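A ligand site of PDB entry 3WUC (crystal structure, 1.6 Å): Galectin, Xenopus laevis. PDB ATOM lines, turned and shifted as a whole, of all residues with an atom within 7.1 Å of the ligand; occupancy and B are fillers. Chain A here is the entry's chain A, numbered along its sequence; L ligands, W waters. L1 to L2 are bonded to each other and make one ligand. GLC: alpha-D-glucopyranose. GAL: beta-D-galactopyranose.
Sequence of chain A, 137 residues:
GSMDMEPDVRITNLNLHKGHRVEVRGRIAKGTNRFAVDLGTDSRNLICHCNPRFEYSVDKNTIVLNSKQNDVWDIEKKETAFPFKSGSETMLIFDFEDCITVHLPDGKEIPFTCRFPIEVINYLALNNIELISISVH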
ATOM      1  N   MET A   3      29.982 -21.531 -20.124  1.00  0.00           N
ATOM      2  CA  MET A   3      28.676 -21.889 -19.496  1.00  0.00           C
ATOM      3  C   MET A   3      28.952 -22.597 -18.159  1.00  0.00           C
ATOM      4  O   MET A   3      30.068 -23.094 -17.944  1.00  0.00           O
ATOM      5  CB  MET A   3      27.872 -22.759 -20.442  1.00  0.00           C
ATOM      6  CG  MET A   3      28.310 -24.236 -20.465  1.00  0.00           C
ATOM      7  SD  MET A   3      27.191 -25.447 -21.199  1.00  0.00           S
ATOM      8  CE  MET A   3      28.349 -26.807 -21.263  1.00  0.00           C
ATOM      9  N   ASP A   4      27.966 -22.682 -17.253  1.00  0.00           N
ATOM     10  CA  ASP A   4      28.183 -23.373 -15.960  1.00  0.00           C
ATOM     11  C   ASP A   4      27.975 -24.887 -15.980  1.00  0.00           C
ATOM     12  O   ASP A   4      28.537 -25.614 -15.205  1.00  0.00           O
ATOM     13  CB  ASP A   4      27.287 -22.824 -14.825  1.00  0.00           C
ATOM     14  CG  ASP A   4      25.803 -22.882 -15.143  1.00  0.00           C
ATOM     15  OD1 ASP A   4      25.542 -22.943 -16.308  1.00  0.00           O
ATOM     16  OD2 ASP A   4      24.918 -22.858 -14.291  1.00  0.00           O
ATOM     17  N   MET A   5      27.097 -25.370 -16.847  1.00  0.00           N
ATOM     18  CA  MET A   5      26.738 -26.756 -16.849  1.00  0.00           C
ATOM     19  C   MET A   5      27.892 -27.668 -17.308  1.00  0.00           C
ATOM     20  O   MET A   5      28.713 -27.224 -18.055  1.00  0.00           O
ATOM     21  CB  MET A   5      25.564 -26.972 -17.874  1.00  0.00           C
ATOM     22  CG  MET A   5      24.253 -26.333 -17.467  1.00  0.00           C
ATOM     23  SD  MET A   5      22.847 -26.630 -18.620  1.00  0.00           S
ATOM     24  CE  MET A   5      23.392 -25.553 -19.957  1.00  0.00           C
ATOM     25  N   ARG A  34      19.813 -27.079 -13.393  1.00  0.00           N
ATOM     26  CA  ARG A  34      19.220 -27.072 -14.702  1.00  0.00           C
ATOM     27  C   ARG A  34      19.962 -28.081 -15.571  1.00  0.00           C
ATOM     28  O   ARG A  34      21.100 -28.428 -15.273  1.00  0.00           O
ATOM     29  CB  ARG A  34      19.293 -25.715 -15.356  1.00  0.00           C
ATOM     30  CG  ARG A  34      20.678 -25.283 -15.828  1.00  0.00           C
ATOM     31  CD  ARG A  34      20.731 -23.760 -15.982  1.00  0.00           C
ATOM     32  NE  ARG A  34      22.043 -23.248 -16.465  1.00  0.00           N
ATOM     33  CZ  ARG A  34      22.217 -22.660 -17.640  1.00  0.00           C
ATOM     34  NH1 ARG A  34      21.292 -22.558 -18.587  1.00  0.00           N
ATOM     35  NH2 ARG A  34      23.438 -22.206 -17.931  1.00  0.00           N
ATOM     36  N   ALA A  36      20.233 -29.221 -20.140  1.00  0.00           N
ATOM     37  CA  ALA A  36      19.817 -28.857 -21.448  1.00  0.00           C
ATOM     38  C   ALA A  36      20.128 -29.899 -22.479  1.00  0.00           C
ATOM     39  O   ALA A  36      21.098 -30.665 -22.324  1.00  0.00           O
ATOM     40  CB  ALA A  36      20.595 -27.635 -21.876  1.00  0.00           C
ATOM     41  N   HIS A  49      17.642 -24.837 -28.058  1.00  0.00           N
ATOM     42  CA  HIS A  49      18.222 -25.009 -26.722  1.00  0.00           C
ATOM     43  C   HIS A  49      17.084 -25.216 -25.788  1.00  0.00           C
ATOM     44  O   HIS A  49      16.234 -24.359 -25.570  1.00  0.00           O
ATOM     45  CB  HIS A  49      18.997 -23.769 -26.350  1.00  0.00           C
ATOM     46  CG  HIS A  49      19.435 -23.666 -24.928  1.00  0.00           C
ATOM     47  ND1 HIS A  49      20.459 -24.375 -24.337  1.00  0.00           N
ATOM     48  CD2 HIS A  49      19.019 -22.810 -23.934  1.00  0.00           C
ATOM     49  CE1 HIS A  49      20.673 -23.973 -23.091  1.00  0.00           C
ATOM     50  NE2 HIS A  49      19.822 -23.000 -22.838  1.00  0.00           N
ATOM     51  N   ASN A  51      16.003 -26.112 -22.201  1.00  0.00           N
ATOM     52  CA  ASN A  51      16.685 -25.925 -20.929  1.00  0.00           C
ATOM     53  C   ASN A  51      15.801 -25.945 -19.663  1.00  0.00           C
ATOM     54  O   ASN A  51      15.369 -24.911 -19.131  1.00  0.00           O
ATOM     55  CB  ASN A  51      17.458 -24.603 -20.955  1.00  0.00           C
ATOM     56  CG  ASN A  51      18.398 -24.390 -19.753  1.00  0.00           C
ATOM     57  OD1 ASN A  51      18.536 -23.216 -19.310  1.00  0.00           O
ATOM     58  ND2 ASN A  51      18.931 -25.453 -19.110  1.00  0.00           N
ATOM     59  N   ARG A  53      14.853 -25.720 -16.035  1.00  0.00           N
ATOM     60  CA  ARG A  53      15.463 -25.145 -14.870  1.00  0.00           C
ATOM     61  C   ARG A  53      14.674 -25.464 -13.635  1.00  0.00           C
ATOM     62  O   ARG A  53      13.511 -25.076 -13.482  1.00  0.00           O
ATOM     63  CB  ARG A  53      15.487 -23.666 -15.087  1.00  0.00           C
ATOM     64  CG  ARG A  53      16.371 -23.227 -16.256  1.00  0.00           C
ATOM     65  CD  ARG A  53      16.229 -21.729 -16.599  1.00  0.00           C
ATOM     66  NE  ARG A  53      17.203 -21.391 -17.653  1.00  0.00           N
ATOM     67  CZ  ARG A  53      17.560 -20.147 -18.006  1.00  0.00           C
ATOM     68  NH1 ARG A  53      17.031 -19.172 -17.340  1.00  0.00           N
ATOM     69  NH2 ARG A  53      18.469 -19.966 -18.924  1.00  0.00           N
ATOM     70  N   TYR A  56      17.173 -21.422 -11.740  1.00  0.00           N
ATOM     71  CA  TYR A  56      18.252 -20.637 -12.318  1.00  0.00           C
ATOM     72  C   TYR A  56      17.703 -19.338 -12.756  1.00  0.00           C
ATOM     73  O   TYR A  56      16.662 -19.235 -13.435  1.00  0.00           O
ATOM     74  CB  TYR A  56      18.874 -21.385 -13.540  1.00  0.00           C
ATOM     75  CG  TYR A  56      20.080 -20.737 -14.188  1.00  0.00           C
ATOM     76  CD1 TYR A  56      21.359 -20.939 -13.643  1.00  0.00           C
ATOM     77  CD2 TYR A  56      19.945 -19.975 -15.317  1.00  0.00           C
ATOM     78  CE1 TYR A  56      22.412 -20.337 -14.242  1.00  0.00           C
ATOM     79  CE2 TYR A  56      21.047 -19.360 -15.927  1.00  0.00           C
ATOM     80  CZ  TYR A  56      22.262 -19.577 -15.387  1.00  0.00           C
ATOM     81  OH  TYR A  56      23.341 -18.945 -16.003  1.00  0.00           O
ATOM     82  N   SER A  57      18.496 -18.296 -12.550  1.00  0.00           N
ATOM     83  CA  SER A  57      18.015 -16.964 -12.807  1.00  0.00           C
ATOM     84  C   SER A  57      16.686 -16.711 -12.102  1.00  0.00           C
ATOM     85  O   SER A  57      16.500 -17.218 -11.010  1.00  0.00           O
ATOM     86  CB  SER A  57      17.985 -16.627 -14.308  1.00  0.00           C
ATOM     87  OG  SER A  57      17.688 -15.231 -14.525  1.00  0.00           O
ATOM     88  N   VAL A  58      15.718 -16.099 -12.803  1.00  0.00           N
ATOM     89  CA  VAL A  58      14.415 -15.857 -12.180  1.00  0.00           C
ATOM     90  C   VAL A  58      13.495 -17.075 -12.319  1.00  0.00           C
ATOM     91  O   VAL A  58      12.361 -17.023 -11.912  1.00  0.00           O
ATOM     92  CB  VAL A  58      13.718 -14.698 -12.896  1.00  0.00           C
ATOM     93  CG1 VAL A  58      14.480 -13.403 -12.618  1.00  0.00           C
ATOM     94  CG2 VAL A  58      13.567 -14.947 -14.377  1.00  0.00           C
ATOM     95  N   ASP A  59      13.968 -18.156 -12.920  1.00  0.00           N
ATOM     96  CA  ASP A  59      13.133 -19.321 -13.200  1.00  0.00           C
ATOM     97  C   ASP A  59      13.210 -20.447 -12.209  1.00  0.00           C
ATOM     98  O   ASP A  59      14.287 -20.908 -11.846  1.00  0.00           O
ATOM     99  CB  ASP A  59      13.507 -19.852 -14.606  1.00  0.00           C
ATOM    100  CG  ASP A  59      13.416 -18.778 -15.634  1.00  0.00           C
ATOM    101  OD1 ASP A  59      12.337 -18.116 -15.766  1.00  0.00           O
ATOM    102  OD2 ASP A  59      14.471 -18.543 -16.272  1.00  0.00           O
ATOM    103  N   VAL A  64      13.046 -23.199 -20.164  1.00  0.00           N
ATOM    104  CA  VAL A  64      13.384 -22.121 -21.127  1.00  0.00           C
ATOM    105  C   VAL A  64      13.775 -22.774 -22.444  1.00  0.00           C
ATOM    106  O   VAL A  64      14.609 -23.732 -22.421  1.00  0.00           O
ATOM    107  CB  VAL A  64      14.557 -21.300 -20.560  1.00  0.00           C
ATOM    108  CG1 VAL A  64      15.272 -20.452 -21.635  1.00  0.00           C
ATOM    109  CG2 VAL A  64      14.115 -20.464 -19.373  1.00  0.00           C
ATOM    110  N   LEU A  65      13.167 -22.290 -23.500  1.00  0.00           N
ATOM    111  CA  LEU A  65      13.606 -22.642 -24.872  1.00  0.00           C
ATOM    112  C   LEU A  65      14.237 -21.419 -25.508  1.00  0.00           C
ATOM    113  O   LEU A  65      13.721 -20.278 -25.364  1.00  0.00           O
ATOM    114  CB  LEU A  65      12.416 -23.076 -25.741  1.00  0.00           C
ATOM    115  CG  LEU A  65      11.665 -24.313 -25.186  1.00  0.00           C
ATOM    116  CD1 LEU A  65      10.464 -24.539 -26.076  1.00  0.00           C
ATOM    117  CD2 LEU A  65      12.484 -25.554 -25.258  1.00  0.00           C
ATOM    118  N   ASN A  66      15.297 -21.559 -26.277  1.00  0.00           N
ATOM    119  CA  ASN A  66      15.890 -20.463 -27.016  1.00  0.00           C
ATOM    120  C   ASN A  66      16.657 -20.994 -28.238  1.00  0.00           C
ATOM    121  O   ASN A  66      16.811 -22.176 -28.428  1.00  0.00           O
ATOM    122  CB  ASN A  66      16.758 -19.595 -26.135  1.00  0.00           C
ATOM    123  CG  ASN A  66      16.813 -18.165 -26.600  1.00  0.00           C
ATOM    124  OD1 ASN A  66      16.361 -17.813 -27.681  1.00  0.00           O
ATOM    125  ND2 ASN A  66      17.437 -17.353 -25.780  1.00  0.00           N
ATOM    126  N   SER A  67      17.072 -20.082 -29.093  1.00  0.00           N
ATOM    127  CA  SER A  67      17.929 -20.300 -30.217  1.00  0.00           C
ATOM    128  C   SER A  67      19.196 -19.420 -30.078  1.00  0.00           C
ATOM    129  O   SER A  67      19.168 -18.456 -29.323  1.00  0.00           O
ATOM    130  CB  SER A  67      17.265 -20.027 -31.560  1.00  0.00           C
ATOM    131  OG  SER A  67      16.650 -18.740 -31.495  1.00  0.00           O
ATOM    132  N   TRP A  73      22.450 -15.356 -28.072  1.00  0.00           N
ATOM    133  CA  TRP A  73      21.125 -15.915 -27.699  1.00  0.00           C
ATOM    134  C   TRP A  73      20.017 -15.014 -28.273  1.00  0.00           C
ATOM    135  O   TRP A  73      20.092 -13.739 -28.257  1.00  0.00           O
ATOM    136  CB  TRP A  73      20.998 -15.994 -26.197  1.00  0.00           C
ATOM    137  CG  TRP A  73      21.814 -17.048 -25.584  1.00  0.00           C
ATOM    138  CD1 TRP A  73      22.936 -16.880 -24.794  1.00  0.00           C
ATOM    139  CD2 TRP A  73      21.655 -18.455 -25.727  1.00  0.00           C
ATOM    140  NE1 TRP A  73      23.440 -18.098 -24.407  1.00  0.00           N
ATOM    141  CE2 TRP A  73      22.676 -19.079 -24.976  1.00  0.00           C
ATOM    142  CE3 TRP A  73      20.733 -19.247 -26.409  1.00  0.00           C
ATOM    143  CZ2 TRP A  73      22.770 -20.452 -24.861  1.00  0.00           C
ATOM    144  CZ3 TRP A  73      20.889 -20.618 -26.331  1.00  0.00           C
ATOM    145  CH2 TRP A  73      21.866 -21.195 -25.547  1.00  0.00           C
ATOM    146  N   ASP A  74      18.969 -15.625 -28.768  1.00  0.00           N
ATOM    147  CA  ASP A  74      17.728 -14.942 -29.177  1.00  0.00           C
ATOM    148  C   ASP A  74      16.812 -14.700 -27.934  1.00  0.00           C
ATOM    149  O   ASP A  74      17.296 -14.659 -26.800  1.00  0.00           O
ATOM    150  CB  ASP A  74      17.088 -15.708 -30.327  1.00  0.00           C
ATOM    151  CG  ASP A  74      17.929 -15.719 -31.579  1.00  0.00           C
ATOM    152  OD1 ASP A  74      18.575 -14.680 -31.904  1.00  0.00           O
ATOM    153  OD2 ASP A  74      18.072 -16.779 -32.245  1.00  0.00           O
ATOM    154  N   ILE A  75      15.524 -14.475 -28.167  1.00  0.00           N
ATOM    155  CA  ILE A  75      14.608 -14.216 -27.091  1.00  0.00           C
ATOM    156  C   ILE A  75      14.039 -15.513 -26.510  1.00  0.00           C
ATOM    157  O   ILE A  75      13.510 -16.330 -27.240  1.00  0.00           O
ATOM    158  CB  ILE A  75      13.489 -13.251 -27.545  1.00  0.00           C
ATOM    159  CG1 ILE A  75      14.152 -11.873 -27.890  1.00  0.00           C
ATOM    160  CG2 ILE A  75      12.521 -13.024 -26.413  1.00  0.00           C
ATOM    161  CD1 ILE A  75      13.674 -11.337 -29.177  1.00  0.00           C
ATOM    162  N   GLU A  76      14.175 -15.689 -25.205  1.00  0.00           N
ATOM    163  CA  GLU A  76      13.673 -16.882 -24.523  1.00  0.00           C
ATOM    164  C   GLU A  76      12.178 -17.045 -24.591  1.00  0.00           C
ATOM    165  O   GLU A  76      11.404 -16.077 -24.523  1.00  0.00           O
ATOM    166  CB  GLU A  76      14.057 -16.899 -23.055  1.00  0.00           C
ATOM    167  CG  GLU A  76      15.506 -16.982 -22.823  1.00  0.00           C
ATOM    168  CD  GLU A  76      15.917 -16.758 -21.398  1.00  0.00           C
ATOM    169  OE1 GLU A  76      15.081 -16.443 -20.507  1.00  0.00           O
ATOM    170  OE2 GLU A  76      17.111 -16.887 -21.180  1.00  0.00           O
ATOM    171  N   LYS A  77      11.715 -18.251 -24.828  1.00  0.00           N
ATOM    172  CA  LYS A  77      10.313 -18.671 -24.625  1.00  0.00           C
ATOM    173  C   LYS A  77      10.215 -19.605 -23.425  1.00  0.00           C
ATOM    174  O   LYS A  77      11.138 -20.431 -23.167  1.00  0.00           O
ATOM    175  CB  LYS A  77       9.852 -19.402 -25.868  1.00  0.00           C
ATOM    176  CG  LYS A  77       9.644 -18.591 -27.119  1.00  0.00           C
ATOM    177  CD  LYS A  77       8.143 -18.184 -27.211  1.00  0.00           C
ATOM    178  CE  LYS A  77       7.807 -17.297 -28.391  1.00  0.00           C
ATOM    179  NZ  LYS A  77       6.375 -16.791 -28.461  1.00  0.00           N
ATOM    180  N   LYS A  78       9.163 -19.468 -22.613  1.00  0.00           N
ATOM    181  CA  LYS A  78       9.182 -20.238 -21.379  1.00  0.00           C
ATOM    182  C   LYS A  78       7.841 -21.022 -21.238  1.00  0.00           C
ATOM    183  O   LYS A  78       6.773 -20.494 -21.616  1.00  0.00           O
ATOM    184  CB  LYS A  78       9.234 -19.338 -20.192  1.00  0.00           C
ATOM    185  CG  LYS A  78      10.455 -18.416 -20.157  1.00  0.00           C
ATOM    186  CD  LYS A  78      10.646 -17.728 -18.842  1.00  0.00           C
ATOM    187  CE  LYS A  78      11.857 -16.803 -18.886  1.00  0.00           C
ATOM    188  NZ  LYS A  78      11.952 -16.180 -17.552  1.00  0.00           N
HETATM  189  C1  GLC L   1      19.090 -13.504 -17.992  1.00  0.00           C
HETATM  190  C2  GLC L   1      18.079 -14.680 -18.146  1.00  0.00           C
HETATM  191  C3  GLC L   1      18.914 -15.970 -18.209  1.00  0.00           C
HETATM  192  C4  GLC L   1      20.134 -15.913 -19.130  1.00  0.00           C
HETATM  193  C5  GLC L   1      21.045 -14.841 -18.551  1.00  0.00           C
HETATM  194  C6  GLC L   1      22.415 -14.770 -19.186  1.00  0.00           C
HETATM  195  O1  GLC L   1      19.469 -13.751 -16.689  1.00  0.00           O
HETATM  196  O2  GLC L   1      17.094 -14.773 -17.146  1.00  0.00           O
HETATM  197  O3  GLC L   1      18.059 -16.957 -18.751  1.00  0.00           O
HETATM  198  O4  GLC L   1      20.883 -17.152 -18.973  1.00  0.00           O
HETATM  199  O5  GLC L   1      20.370 -13.601 -18.579  1.00  0.00           O
HETATM  200  O6  GLC L   1      22.166 -14.178 -20.427  1.00  0.00           O
HETATM  201  C1  GAL L   2      21.347 -17.777 -20.149  1.00  0.00           C
HETATM  202  C2  GAL L   2      22.252 -18.960 -19.753  1.00  0.00           C
HETATM  203  C3  GAL L   2      22.514 -19.872 -20.949  1.00  0.00           C
HETATM  204  C4  GAL L   2      21.206 -20.187 -21.724  1.00  0.00           C
HETATM  205  C5  GAL L   2      20.467 -18.899 -22.016  1.00  0.00           C
HETATM  206  C6  GAL L   2      19.158 -19.149 -22.764  1.00  0.00           C
HETATM  207  O2  GAL L   2      23.470 -18.531 -19.088  1.00  0.00           O
HETATM  208  O3  GAL L   2      23.265 -21.013 -20.567  1.00  0.00           O
HETATM  209  O4  GAL L   2      20.430 -21.131 -20.973  1.00  0.00           O
HETATM  210  O5  GAL L   2      20.178 -18.241 -20.783  1.00  0.00           O
HETATM  211  O6  GAL L   2      18.506 -17.956 -23.134  1.00  0.00           O
HETATM  212  O   HOH W   1      15.611 -12.443 -16.925  1.00  0.00           O
HETATM  213  O   HOH W   2      15.030 -16.242 -17.786  1.00  0.00           O
HETATM  214  O   HOH W   3      25.116 -16.875 -20.765  1.00  0.00           O
HETATM  215  O   HOH W   4      19.789 -15.402 -22.929  1.00  0.00           O
HETATM  216  O   HOH W   5      19.824 -11.326 -15.323  1.00  0.00           O
HETATM  217  O   HOH W   6      25.900 -19.876 -19.367  1.00  0.00           O
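A ring nitrogen (NE2) of His 49 lies within hydrogen-bond range of an oxygen (O4) of GAL L2 (2.7 Å). The guanidinium group (NH1) of Arg 53 is in hydrogen-bond range of an oxygen (O3) of GLC L1 (2.8 Å). The side-chain carboxylate (OE2) of Glu 76 lies within hydrogen-bond range of an oxygen (O3) of GLC L1, at 2.6 Å. The side-chain amide oxygen of Asn 51 is in hydrogen-bond range of an oxygen (O4) of GAL L2, at 3.3 Å. An oxygen (O3) of GAL L2 lies within hydrogen-bond range of the guanidinium group (NH2) of Arg 34. The side-chain hydroxyl (OH) of Tyr 56 lies within hydrogen-bond range of an oxygen (O2) of GAL L2. An oxygen (O6) of GAL L2 sits at hydrogen-bond distance from the side-chain amide nitrogen (ND2) of Asn 66 (2.9 Å). O2 of GLC L1 lies within hydrogen-bond range of OG of Ser 57.
The side-chain amide nitrogen (ND2) of Asn 66 sits at hydrogen-bond distance from the backbone carbonyl oxygen (O) of Asp 74, at 2.9 Å. The guanidinium group (NH2) of Arg 34 lies within salt-bridge range of the side-chain carboxylate (OD1) of Asp 4. The side-chain amide oxygen of Asn 51 is in hydrogen-bond range of the guanidinium group of Arg 34 (2.9 Å). N of His 49 lies within hydrogen-bond range of O of Asn 66. NH1 of Arg 53 is in salt-bridge range of OD2 of Asp 59, at 2.8 Å. The side-chain amide oxygen (OD1) of Asn 66 sits close to the backbone carbonyl oxygen (O) of Ile 75. NE of Arg 53 sits at hydrogen-bond distance from OD1 of Asn 51 (2.8 Å). The backbone NH of Asn 51 is in hydrogen-bond range of the backbone carbonyl oxygen of Val 64.
Residues that only touch the ligand: Trp 73 (3.5 Å). Hydrophobic or aromatic side chains within 4 Å of the ligand: His 49, Tyr 56 and Trp 73. Within 4 Å of the ligand: Arg 34, His 49, Asn 51, Arg 53, Tyr 56, Ser 57, Asn 66, Trp 73 and Glu 76. Along chain A the residues within 4 Å of the ligand span positions 34 to 76.
Water W2 lies within hydrogen-bond range of an oxygen (O2) of GLC L1, the side-chain carboxylate of Glu 76, the side-chain carboxylate of Asp 59 and the side-chain amino group of Lys 78.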
